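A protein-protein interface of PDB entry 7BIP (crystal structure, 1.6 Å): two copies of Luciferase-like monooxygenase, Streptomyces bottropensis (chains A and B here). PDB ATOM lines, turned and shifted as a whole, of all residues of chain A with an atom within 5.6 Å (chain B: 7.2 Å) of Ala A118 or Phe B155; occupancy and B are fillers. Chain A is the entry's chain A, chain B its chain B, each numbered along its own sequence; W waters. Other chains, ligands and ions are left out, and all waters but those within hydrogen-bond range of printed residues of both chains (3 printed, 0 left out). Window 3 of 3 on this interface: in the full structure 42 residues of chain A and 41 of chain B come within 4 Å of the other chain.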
ATOM      1  N   PHE A  47     -19.110  21.724 -22.062  1.00  0.00           N
ATOM      2  CA  PHE A  47     -18.742  23.147 -22.058  1.00  0.00           C
ATOM      3  C   PHE A  47     -17.681  23.570 -21.048  1.00  0.00           C
ATOM      4  O   PHE A  47     -16.982  24.560 -21.281  1.00  0.00           O
ATOM      5  CB  PHE A  47     -19.956  24.059 -21.826  1.00  0.00           C
ATOM      6  CG  PHE A  47     -21.137  23.740 -22.678  1.00  0.00           C
ATOM      7  CD1 PHE A  47     -20.994  23.440 -24.023  1.00  0.00           C
ATOM      8  CD2 PHE A  47     -22.401  23.740 -22.123  1.00  0.00           C
ATOM      9  CE1 PHE A  47     -22.090  23.138 -24.795  1.00  0.00           C
ATOM     10  CE2 PHE A  47     -23.499  23.453 -22.887  1.00  0.00           C
ATOM     11  CZ  PHE A  47     -23.348  23.147 -24.231  1.00  0.00           C
ATOM     12  N   PRO A 113     -26.269  23.815 -14.648  1.00  0.00           N
ATOM     13  CA  PRO A 113     -27.297  24.694 -15.234  1.00  0.00           C
ATOM     14  C   PRO A 113     -27.011  25.098 -16.671  1.00  0.00           C
ATOM     15  O   PRO A 113     -27.944  25.175 -17.479  1.00  0.00           O
ATOM     16  CB  PRO A 113     -27.301  25.900 -14.283  1.00  0.00           C
ATOM     17  CG  PRO A 113     -26.799  25.341 -12.980  1.00  0.00           C
ATOM     18  CD  PRO A 113     -25.753  24.336 -13.370  1.00  0.00           C
ATOM     19  N   ASP A 114     -25.744  25.331 -17.026  1.00  0.00           N
ATOM     20  CA  ASP A 114     -25.438  25.718 -18.400  1.00  0.00           C
ATOM     21  C   ASP A 114     -25.774  24.616 -19.398  1.00  0.00           C
ATOM     22  O   ASP A 114     -26.081  24.910 -20.559  1.00  0.00           O
ATOM     23  CB  ASP A 114     -23.967  26.105 -18.532  1.00  0.00           C
ATOM     24  CG  ASP A 114     -23.640  27.389 -17.801  1.00  0.00           C
ATOM     25  OD1 ASP A 114     -22.444  27.712 -17.665  1.00  0.00           O
ATOM     26  OD2 ASP A 114     -24.585  28.072 -17.355  1.00  0.00           O
ATOM     27  N   GLU A 115     -25.686  23.345 -18.991  1.00  0.00           N
ATOM     28  CA  GLU A 115     -26.095  22.272 -19.895  1.00  0.00           C
ATOM     29  C   GLU A 115     -27.579  22.369 -20.212  1.00  0.00           C
ATOM     30  O   GLU A 115     -27.977  22.287 -21.378  1.00  0.00           O
ATOM     31  CB  GLU A 115     -25.749  20.901 -19.305  1.00  0.00           C
ATOM     32  CG  GLU A 115     -24.248  20.658 -19.178  1.00  0.00           C
ATOM     33  CD  GLU A 115     -23.893  19.363 -18.462  1.00  0.00           C
ATOM     34  OE1 GLU A 115     -24.778  18.769 -17.800  1.00  0.00           O
ATOM     35  OE2 GLU A 115     -22.710  18.959 -18.539  1.00  0.00           O
ATOM     36  N   PHE A 116     -28.421  22.569 -19.189  1.00  0.00           N
ATOM     37  CA  PHE A 116     -29.856  22.713 -19.430  1.00  0.00           C
ATOM     38  C   PHE A 116     -30.155  23.937 -20.290  1.00  0.00           C
ATOM     39  O   PHE A 116     -30.988  23.879 -21.208  1.00  0.00           O
ATOM     40  CB  PHE A 116     -30.611  22.821 -18.098  1.00  0.00           C
ATOM     41  CG  PHE A 116     -30.815  21.499 -17.400  1.00  0.00           C
ATOM     42  CD1 PHE A 116     -31.903  20.695 -17.713  1.00  0.00           C
ATOM     43  CD2 PHE A 116     -29.926  21.073 -16.413  1.00  0.00           C
ATOM     44  CE1 PHE A 116     -32.094  19.476 -17.067  1.00  0.00           C
ATOM     45  CE2 PHE A 116     -30.115  19.867 -15.761  1.00  0.00           C
ATOM     46  CZ  PHE A 116     -31.198  19.069 -16.084  1.00  0.00           C
ATOM     47  N   THR A 117     -29.504  25.062 -19.992  1.00  0.00           N
ATOM     48  CA  THR A 117     -29.801  26.291 -20.718  1.00  0.00           C
ATOM     49  C   THR A 117     -29.429  26.158 -22.187  1.00  0.00           C
ATOM     50  O   THR A 117     -30.198  26.558 -23.074  1.00  0.00           O
ATOM     51  CB  THR A 117     -29.058  27.471 -20.094  1.00  0.00           C
ATOM     52  OG1 THR A 117     -29.456  27.624 -18.727  1.00  0.00           O
ATOM     53  CG2 THR A 117     -29.390  28.741 -20.856  1.00  0.00           C
ATOM     54  N   ALA A 118     -28.259  25.584 -22.464  1.00  0.00           N
ATOM     55  CA  ALA A 118     -27.779  25.511 -23.841  1.00  0.00           C
ATOM     56  C   ALA A 118     -28.642  24.590 -24.690  1.00  0.00           C
ATOM     57  O   ALA A 118     -28.887  24.870 -25.869  1.00  0.00           O
ATOM     58  CB  ALA A 118     -26.322  25.052 -23.866  1.00  0.00           C
ATOM     59  N   PHE A 119     -29.115  23.486 -24.116  1.00  0.00           N
ATOM     60  CA  PHE A 119     -29.985  22.587 -24.862  1.00  0.00           C
ATOM     61  C   PHE A 119     -31.445  23.015 -24.804  1.00  0.00           C
ATOM     62  O   PHE A 119     -32.292  22.360 -25.421  1.00  0.00           O
ATOM     63  CB  PHE A 119     -29.818  21.152 -24.353  1.00  0.00           C
ATOM     64  CG  PHE A 119     -28.563  20.480 -24.841  1.00  0.00           C
ATOM     65  CD1 PHE A 119     -28.503  19.955 -26.116  1.00  0.00           C
ATOM     66  CD2 PHE A 119     -27.446  20.360 -24.017  1.00  0.00           C
ATOM     67  CE1 PHE A 119     -27.354  19.326 -26.575  1.00  0.00           C
ATOM     68  CE2 PHE A 119     -26.289  19.723 -24.466  1.00  0.00           C
ATOM     69  CZ  PHE A 119     -26.246  19.212 -25.750  1.00  0.00           C
ATOM     70  N   GLU A 120     -31.739  24.123 -24.122  1.00  0.00           N
ATOM     71  CA  GLU A 120     -33.088  24.682 -24.041  1.00  0.00           C
ATOM     72  C   GLU A 120     -34.065  23.656 -23.477  1.00  0.00           C
ATOM     73  O   GLU A 120     -35.177  23.473 -23.983  1.00  0.00           O
ATOM     74  CB  GLU A 120     -33.558  25.206 -25.404  1.00  0.00           C
ATOM     75  CG  GLU A 120     -32.674  26.334 -25.944  1.00  0.00           C
ATOM     76  CD  GLU A 120     -33.112  26.795 -27.321  1.00  0.00           C
ATOM     77  OE1 GLU A 120     -33.906  27.762 -27.404  1.00  0.00           O
ATOM     78  OE2 GLU A 120     -32.673  26.188 -28.321  1.00  0.00           O
ATOM     79  N   HIS B  84     -28.725  17.589 -32.483  1.00  0.00           N
ATOM     80  CA  HIS B  84     -28.461  18.962 -32.088  1.00  0.00           C
ATOM     81  C   HIS B  84     -27.025  19.337 -32.456  1.00  0.00           C
ATOM     82  O   HIS B  84     -26.114  18.531 -32.289  1.00  0.00           O
ATOM     83  CB  HIS B  84     -28.681  19.102 -30.585  1.00  0.00           C
ATOM     84  CG  HIS B  84     -28.767  20.512 -30.097  1.00  0.00           C
ATOM     85  ND1 HIS B  84     -27.693  21.373 -30.116  1.00  0.00           N
ATOM     86  CD2 HIS B  84     -29.786  21.193 -29.519  1.00  0.00           C
ATOM     87  CE1 HIS B  84     -28.056  22.538 -29.608  1.00  0.00           C
ATOM     88  NE2 HIS B  84     -29.321  22.454 -29.233  1.00  0.00           N
ATOM     89  N   PRO B  85     -26.793  20.549 -32.965  1.00  0.00           N
ATOM     90  CA  PRO B  85     -25.422  20.929 -33.338  1.00  0.00           C
ATOM     91  C   PRO B  85     -24.440  20.861 -32.184  1.00  0.00           C
ATOM     92  O   PRO B  85     -23.264  20.565 -32.413  1.00  0.00           O
ATOM     93  CB  PRO B  85     -25.580  22.366 -33.872  1.00  0.00           C
ATOM     94  CG  PRO B  85     -26.930  22.803 -33.436  1.00  0.00           C
ATOM     95  CD  PRO B  85     -27.779  21.569 -33.345  1.00  0.00           C
ATOM     96  N   LEU B  86     -24.876  21.108 -30.948  1.00  0.00           N
ATOM     97  CA  LEU B  86     -23.959  20.986 -29.819  1.00  0.00           C
ATOM     98  C   LEU B  86     -23.440  19.563 -29.680  1.00  0.00           C
ATOM     99  O   LEU B  86     -22.243  19.353 -29.446  1.00  0.00           O
ATOM    100  CB  LEU B  86     -24.644  21.421 -28.525  1.00  0.00           C
ATOM    101  CG  LEU B  86     -24.900  22.930 -28.388  1.00  0.00           C
ATOM    102  CD1 LEU B  86     -25.796  23.187 -27.184  1.00  0.00           C
ATOM    103  CD2 LEU B  86     -23.595  23.722 -28.278  1.00  0.00           C
ATOM    104  N   ALA B 136     -23.729  26.009 -37.652  1.00  0.00           N
ATOM    105  CA  ALA B 136     -23.540  26.080 -36.207  1.00  0.00           C
ATOM    106  C   ALA B 136     -22.392  25.187 -35.767  1.00  0.00           C
ATOM    107  O   ALA B 136     -21.589  25.577 -34.914  1.00  0.00           O
ATOM    108  CB  ALA B 136     -24.827  25.702 -35.467  1.00  0.00           C
ATOM    109  N   VAL B 137     -22.296  23.979 -36.335  1.00  0.00           N
ATOM    110  CA  VAL B 137     -21.195  23.090 -35.976  1.00  0.00           C
ATOM    111  C   VAL B 137     -19.859  23.717 -36.357  1.00  0.00           C
ATOM    112  O   VAL B 137     -18.908  23.726 -35.561  1.00  0.00           O
ATOM    113  CB  VAL B 137     -21.383  21.710 -36.635  1.00  0.00           C
ATOM    114  CG1 VAL B 137     -20.119  20.867 -36.442  1.00  0.00           C
ATOM    115  CG2 VAL B 137     -22.591  20.998 -36.029  1.00  0.00           C
ATOM    116  N   LEU B 140     -18.940  26.305 -33.831  1.00  0.00           N
ATOM    117  CA  LEU B 140     -18.586  25.715 -32.543  1.00  0.00           C
ATOM    118  C   LEU B 140     -17.154  25.198 -32.549  1.00  0.00           C
ATOM    119  O   LEU B 140     -16.466  25.257 -31.519  1.00  0.00           O
ATOM    120  CB  LEU B 140     -19.559  24.588 -32.201  1.00  0.00           C
ATOM    121  CG  LEU B 140     -20.929  25.074 -31.732  1.00  0.00           C
ATOM    122  CD1 LEU B 140     -21.985  23.996 -31.895  1.00  0.00           C
ATOM    123  CD2 LEU B 140     -20.850  25.555 -30.278  1.00  0.00           C
ATOM    124  N   VAL B 146     -19.192  31.088 -28.412  1.00  0.00           N
ATOM    125  CA  VAL B 146     -20.099  31.084 -29.555  1.00  0.00           C
ATOM    126  C   VAL B 146     -21.526  31.311 -29.078  1.00  0.00           C
ATOM    127  O   VAL B 146     -21.997  30.653 -28.142  1.00  0.00           O
ATOM    128  CB  VAL B 146     -19.983  29.758 -30.325  1.00  0.00           C
ATOM    129  CG1 VAL B 146     -21.166  29.564 -31.275  1.00  0.00           C
ATOM    130  CG2 VAL B 146     -18.664  29.712 -31.072  1.00  0.00           C
ATOM    131  N   VAL B 147     -22.217  32.253 -29.705  1.00  0.00           N
ATOM    132  CA  VAL B 147     -23.657  32.418 -29.531  1.00  0.00           C
ATOM    133  C   VAL B 147     -24.290  32.135 -30.887  1.00  0.00           C
ATOM    134  O   VAL B 147     -23.855  32.682 -31.911  1.00  0.00           O
ATOM    135  CB  VAL B 147     -24.037  33.824 -29.022  1.00  0.00           C
ATOM    136  CG1 VAL B 147     -25.547  33.922 -28.788  1.00  0.00           C
ATOM    137  CG2 VAL B 147     -23.293  34.195 -27.736  1.00  0.00           C
ATOM    138  N   TRP B 148     -25.288  31.261 -30.902  1.00  0.00           N
ATOM    139  CA  TRP B 148     -25.992  30.893 -32.123  1.00  0.00           C
ATOM    140  C   TRP B 148     -27.474  31.082 -31.861  1.00  0.00           C
ATOM    141  O   TRP B 148     -28.007  30.529 -30.891  1.00  0.00           O
ATOM    142  CB  TRP B 148     -25.709  29.438 -32.531  1.00  0.00           C
ATOM    143  CG  TRP B 148     -26.579  28.977 -33.656  1.00  0.00           C
ATOM    144  CD1 TRP B 148     -27.771  28.311 -33.559  1.00  0.00           C
ATOM    145  CD2 TRP B 148     -26.348  29.187 -35.051  1.00  0.00           C
ATOM    146  NE1 TRP B 148     -28.286  28.082 -34.814  1.00  0.00           N
ATOM    147  CE2 TRP B 148     -27.431  28.611 -35.747  1.00  0.00           C
ATOM    148  CE3 TRP B 148     -25.320  29.792 -35.784  1.00  0.00           C
ATOM    149  CZ2 TRP B 148     -27.515  28.629 -37.139  1.00  0.00           C
ATOM    150  CZ3 TRP B 148     -25.404  29.810 -37.158  1.00  0.00           C
ATOM    151  CH2 TRP B 148     -26.499  29.246 -37.825  1.00  0.00           C
ATOM    152  N   GLU B 149     -28.142  31.861 -32.716  1.00  0.00           N
ATOM    153  CA  GLU B 149     -29.570  32.134 -32.541  1.00  0.00           C
ATOM    154  C   GLU B 149     -30.244  31.939 -33.886  1.00  0.00           C
ATOM    155  O   GLU B 149     -30.483  32.894 -34.634  1.00  0.00           O
ATOM    156  CB  GLU B 149     -29.803  33.526 -31.960  1.00  0.00           C
ATOM    157  CG  GLU B 149     -29.543  33.526 -30.455  1.00  0.00           C
ATOM    158  CD  GLU B 149     -29.411  34.907 -29.856  1.00  0.00           C
ATOM    159  OE1 GLU B 149     -29.223  35.894 -30.600  1.00  0.00           O
ATOM    160  OE2 GLU B 149     -29.483  35.002 -28.623  1.00  0.00           O
ATOM    161  N   GLY B 150     -30.545  30.682 -34.190  1.00  0.00           N
ATOM    162  CA  GLY B 150     -31.109  30.299 -35.461  1.00  0.00           C
ATOM    163  C   GLY B 150     -32.610  30.096 -35.404  1.00  0.00           C
ATOM    164  O   GLY B 150     -33.309  30.615 -34.523  1.00  0.00           O
ATOM    165  N   HIS B 153     -32.462  26.324 -32.974  1.00  0.00           N
ATOM    166  CA  HIS B 153     -31.717  26.266 -31.729  1.00  0.00           C
ATOM    167  C   HIS B 153     -31.173  27.637 -31.389  1.00  0.00           C
ATOM    168  O   HIS B 153     -30.780  28.392 -32.279  1.00  0.00           O
ATOM    169  CB  HIS B 153     -30.563  25.271 -31.829  1.00  0.00           C
ATOM    170  CG  HIS B 153     -31.002  23.913 -32.252  1.00  0.00           C
ATOM    171  ND1 HIS B 153     -30.754  23.406 -33.509  1.00  0.00           N
ATOM    172  CD2 HIS B 153     -31.722  22.971 -31.598  1.00  0.00           C
ATOM    173  CE1 HIS B 153     -31.278  22.196 -33.601  1.00  0.00           C
ATOM    174  NE2 HIS B 153     -31.865  21.906 -32.454  1.00  0.00           N
ATOM    175  N   ARG B 154     -31.157  27.947 -30.097  1.00  0.00           N
ATOM    176  CA  ARG B 154     -30.604  29.196 -29.590  1.00  0.00           C
ATOM    177  C   ARG B 154     -29.769  28.856 -28.368  1.00  0.00           C
ATOM    178  O   ARG B 154     -30.304  28.306 -27.401  1.00  0.00           O
ATOM    179  CB  ARG B 154     -31.712  30.188 -29.224  1.00  0.00           C
ATOM    180  CG  ARG B 154     -32.532  30.669 -30.404  1.00  0.00           C
ATOM    181  CD  ARG B 154     -34.014  30.628 -30.076  1.00  0.00           C
ATOM    182  NE  ARG B 154     -34.391  29.255 -29.750  1.00  0.00           N
ATOM    183  CZ  ARG B 154     -35.001  28.430 -30.592  1.00  0.00           C
ATOM    184  NH1 ARG B 154     -35.329  28.841 -31.814  1.00  0.00           N
ATOM    185  NH2 ARG B 154     -35.283  27.192 -30.208  1.00  0.00           N
ATOM    186  N   PHE B 155     -28.475  29.183 -28.399  1.00  0.00           N
ATOM    187  CA  PHE B 155     -27.612  28.890 -27.257  1.00  0.00           C
ATOM    188  C   PHE B 155     -26.402  29.815 -27.242  1.00  0.00           C
ATOM    189  O   PHE B 155     -26.031  30.411 -28.256  1.00  0.00           O
ATOM    190  CB  PHE B 155     -27.137  27.431 -27.271  1.00  0.00           C
ATOM    191  CG  PHE B 155     -26.522  27.005 -28.571  1.00  0.00           C
ATOM    192  CD1 PHE B 155     -25.190  27.295 -28.865  1.00  0.00           C
ATOM    193  CD2 PHE B 155     -27.273  26.317 -29.506  1.00  0.00           C
ATOM    194  CE1 PHE B 155     -24.623  26.897 -30.084  1.00  0.00           C
ATOM    195  CE2 PHE B 155     -26.719  25.908 -30.724  1.00  0.00           C
ATOM    196  CZ  PHE B 155     -25.392  26.202 -31.014  1.00  0.00           C
ATOM    197  N   GLY B 156     -25.773  29.904 -26.071  1.00  0.00           N
ATOM    198  CA  GLY B 156     -24.509  30.592 -25.946  1.00  0.00           C
ATOM    199  C   GLY B 156     -24.529  31.720 -24.941  1.00  0.00           C
ATOM    200  O   GLY B 156     -25.588  32.138 -24.464  1.00  0.00           O
ATOM    201  N   PRO B 157     -23.346  32.267 -24.615  1.00  0.00           N
ATOM    202  CA  PRO B 157     -22.050  31.888 -25.196  1.00  0.00           C
ATOM    203  C   PRO B 157     -21.519  30.566 -24.652  1.00  0.00           C
ATOM    204  O   PRO B 157     -21.625  30.310 -23.448  1.00  0.00           O
ATOM    205  CB  PRO B 157     -21.125  33.035 -24.790  1.00  0.00           C
ATOM    206  CG  PRO B 157     -21.749  33.601 -23.557  1.00  0.00           C
ATOM    207  CD  PRO B 157     -23.234  33.424 -23.707  1.00  0.00           C
ATOM    208  N   VAL B 158     -20.987  29.729 -25.535  1.00  0.00           N
ATOM    209  CA  VAL B 158     -20.353  28.478 -25.133  1.00  0.00           C
ATOM    210  C   VAL B 158     -19.058  28.310 -25.912  1.00  0.00           C
ATOM    211  O   VAL B 158     -18.934  28.742 -27.063  1.00  0.00           O
ATOM    212  CB  VAL B 158     -21.258  27.240 -25.354  1.00  0.00           C
ATOM    213  CG1 VAL B 158     -22.448  27.259 -24.403  1.00  0.00           C
ATOM    214  CG2 VAL B 158     -21.708  27.148 -26.800  1.00  0.00           C
ATOM    215  N   MET B 160     -17.164  25.118 -27.137  1.00  0.00           N
ATOM    216  CA  MET B 160     -17.361  23.682 -27.221  1.00  0.00           C
ATOM    217  C   MET B 160     -16.041  22.974 -26.949  1.00  0.00           C
ATOM    218  O   MET B 160     -15.010  23.311 -27.538  1.00  0.00           O
ATOM    219  CB  MET B 160     -17.918  23.290 -28.595  1.00  0.00           C
ATOM    220  CG  MET B 160     -18.071  21.755 -28.803  1.00  0.00           C
ATOM    221  SD  MET B 160     -19.075  20.858 -27.574  1.00  0.00           S
ATOM    222  CE  MET B 160     -20.509  21.909 -27.555  1.00  0.00           C
HETATM  223  O   HOH W   1     -30.092  28.695 -24.682  1.00  0.00           O
HETATM  224  O   HOH W   2     -30.460  24.750 -28.144  1.00  0.00           O
HETATM  225  O   HOH W   3     -18.123  19.921 -24.164  1.00  0.00           O
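No position is printed for both chains. Of the 8 pairs that touch across the chains among the printed residues, none has its exchanged pair printed and touching as well.
Printed residues of chain B that touch a printed residue of chain A: His B84, Leu B86, His B153, Arg B154, Phe B155 and Met B160. Hydrophobic or aromatic side chains of chain B within 4 Å of the printed part of chain A: His B84, Leu B86, Phe B155 and Met B160. Among the printed residues, 8 pairs touch across the chains. Among the printed residues, Asp or Glu carboxylates within 4 Å of a Lys or Arg side-chain nitrogen of the other chain: Glu A120 with Arg B154.
Water W2 lies within hydrogen-bond range of OE2 of Glu A120, O of Ala A118 and NE2 of His B84. Water W1 lies within hydrogen-bond range of O of Thr A117 (2.7 Å) and O of Arg B154 (2.8 Å). Water W3 lies within hydrogen-bond range of the backbone NH of Phe A47 (2.9 Å) and the side-chain sulfur of Met B160 (3.7 Å).
NE of Arg B154 lies within salt-bridge range of OE1 of Glu A120 (2.8 Å).
Ala A118 touches two residues of chain B. Of chain A, only Ala A118 (3.4 Å) comes within 4 Å of Phe B155. Printed residues of chain B within 4 Å of Glu A120: His B153 and Arg B154. Of the printed residues of chain B, Phe A47 touches Leu B86 (3.8 Å) and Met B160 (3.4 Å). Printed residues of chain A within 4 Å of Met B160: Phe A47 (3.4 Å). Thr A117 touches none of the printed residues of chain B. Gly B150 touches none of the printed residues of chain A. The nearest residue of chain B that does not touch Ala A118 is Arg B154 (4.02 Å). The nearest printed residue of chain A that does not touch His B153 is Ala A118 (6.2 Å).
Among the printed residues, merely in contact across the chains: Ala A118 with Phe B155, Phe A47 with Met B160, Glu A120 with His B153, Ala A118 with Leu B86, Phe A47 with Leu B86, Phe A119 with His B84 and Phe A119 with Leu B86.
ND1 of His B84 sits at hydrogen-bond distance from N of Leu B86, at 2.9 Å. N of Phe B155 is in hydrogen-bond range of O of Trp B148 (2.9 Å).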
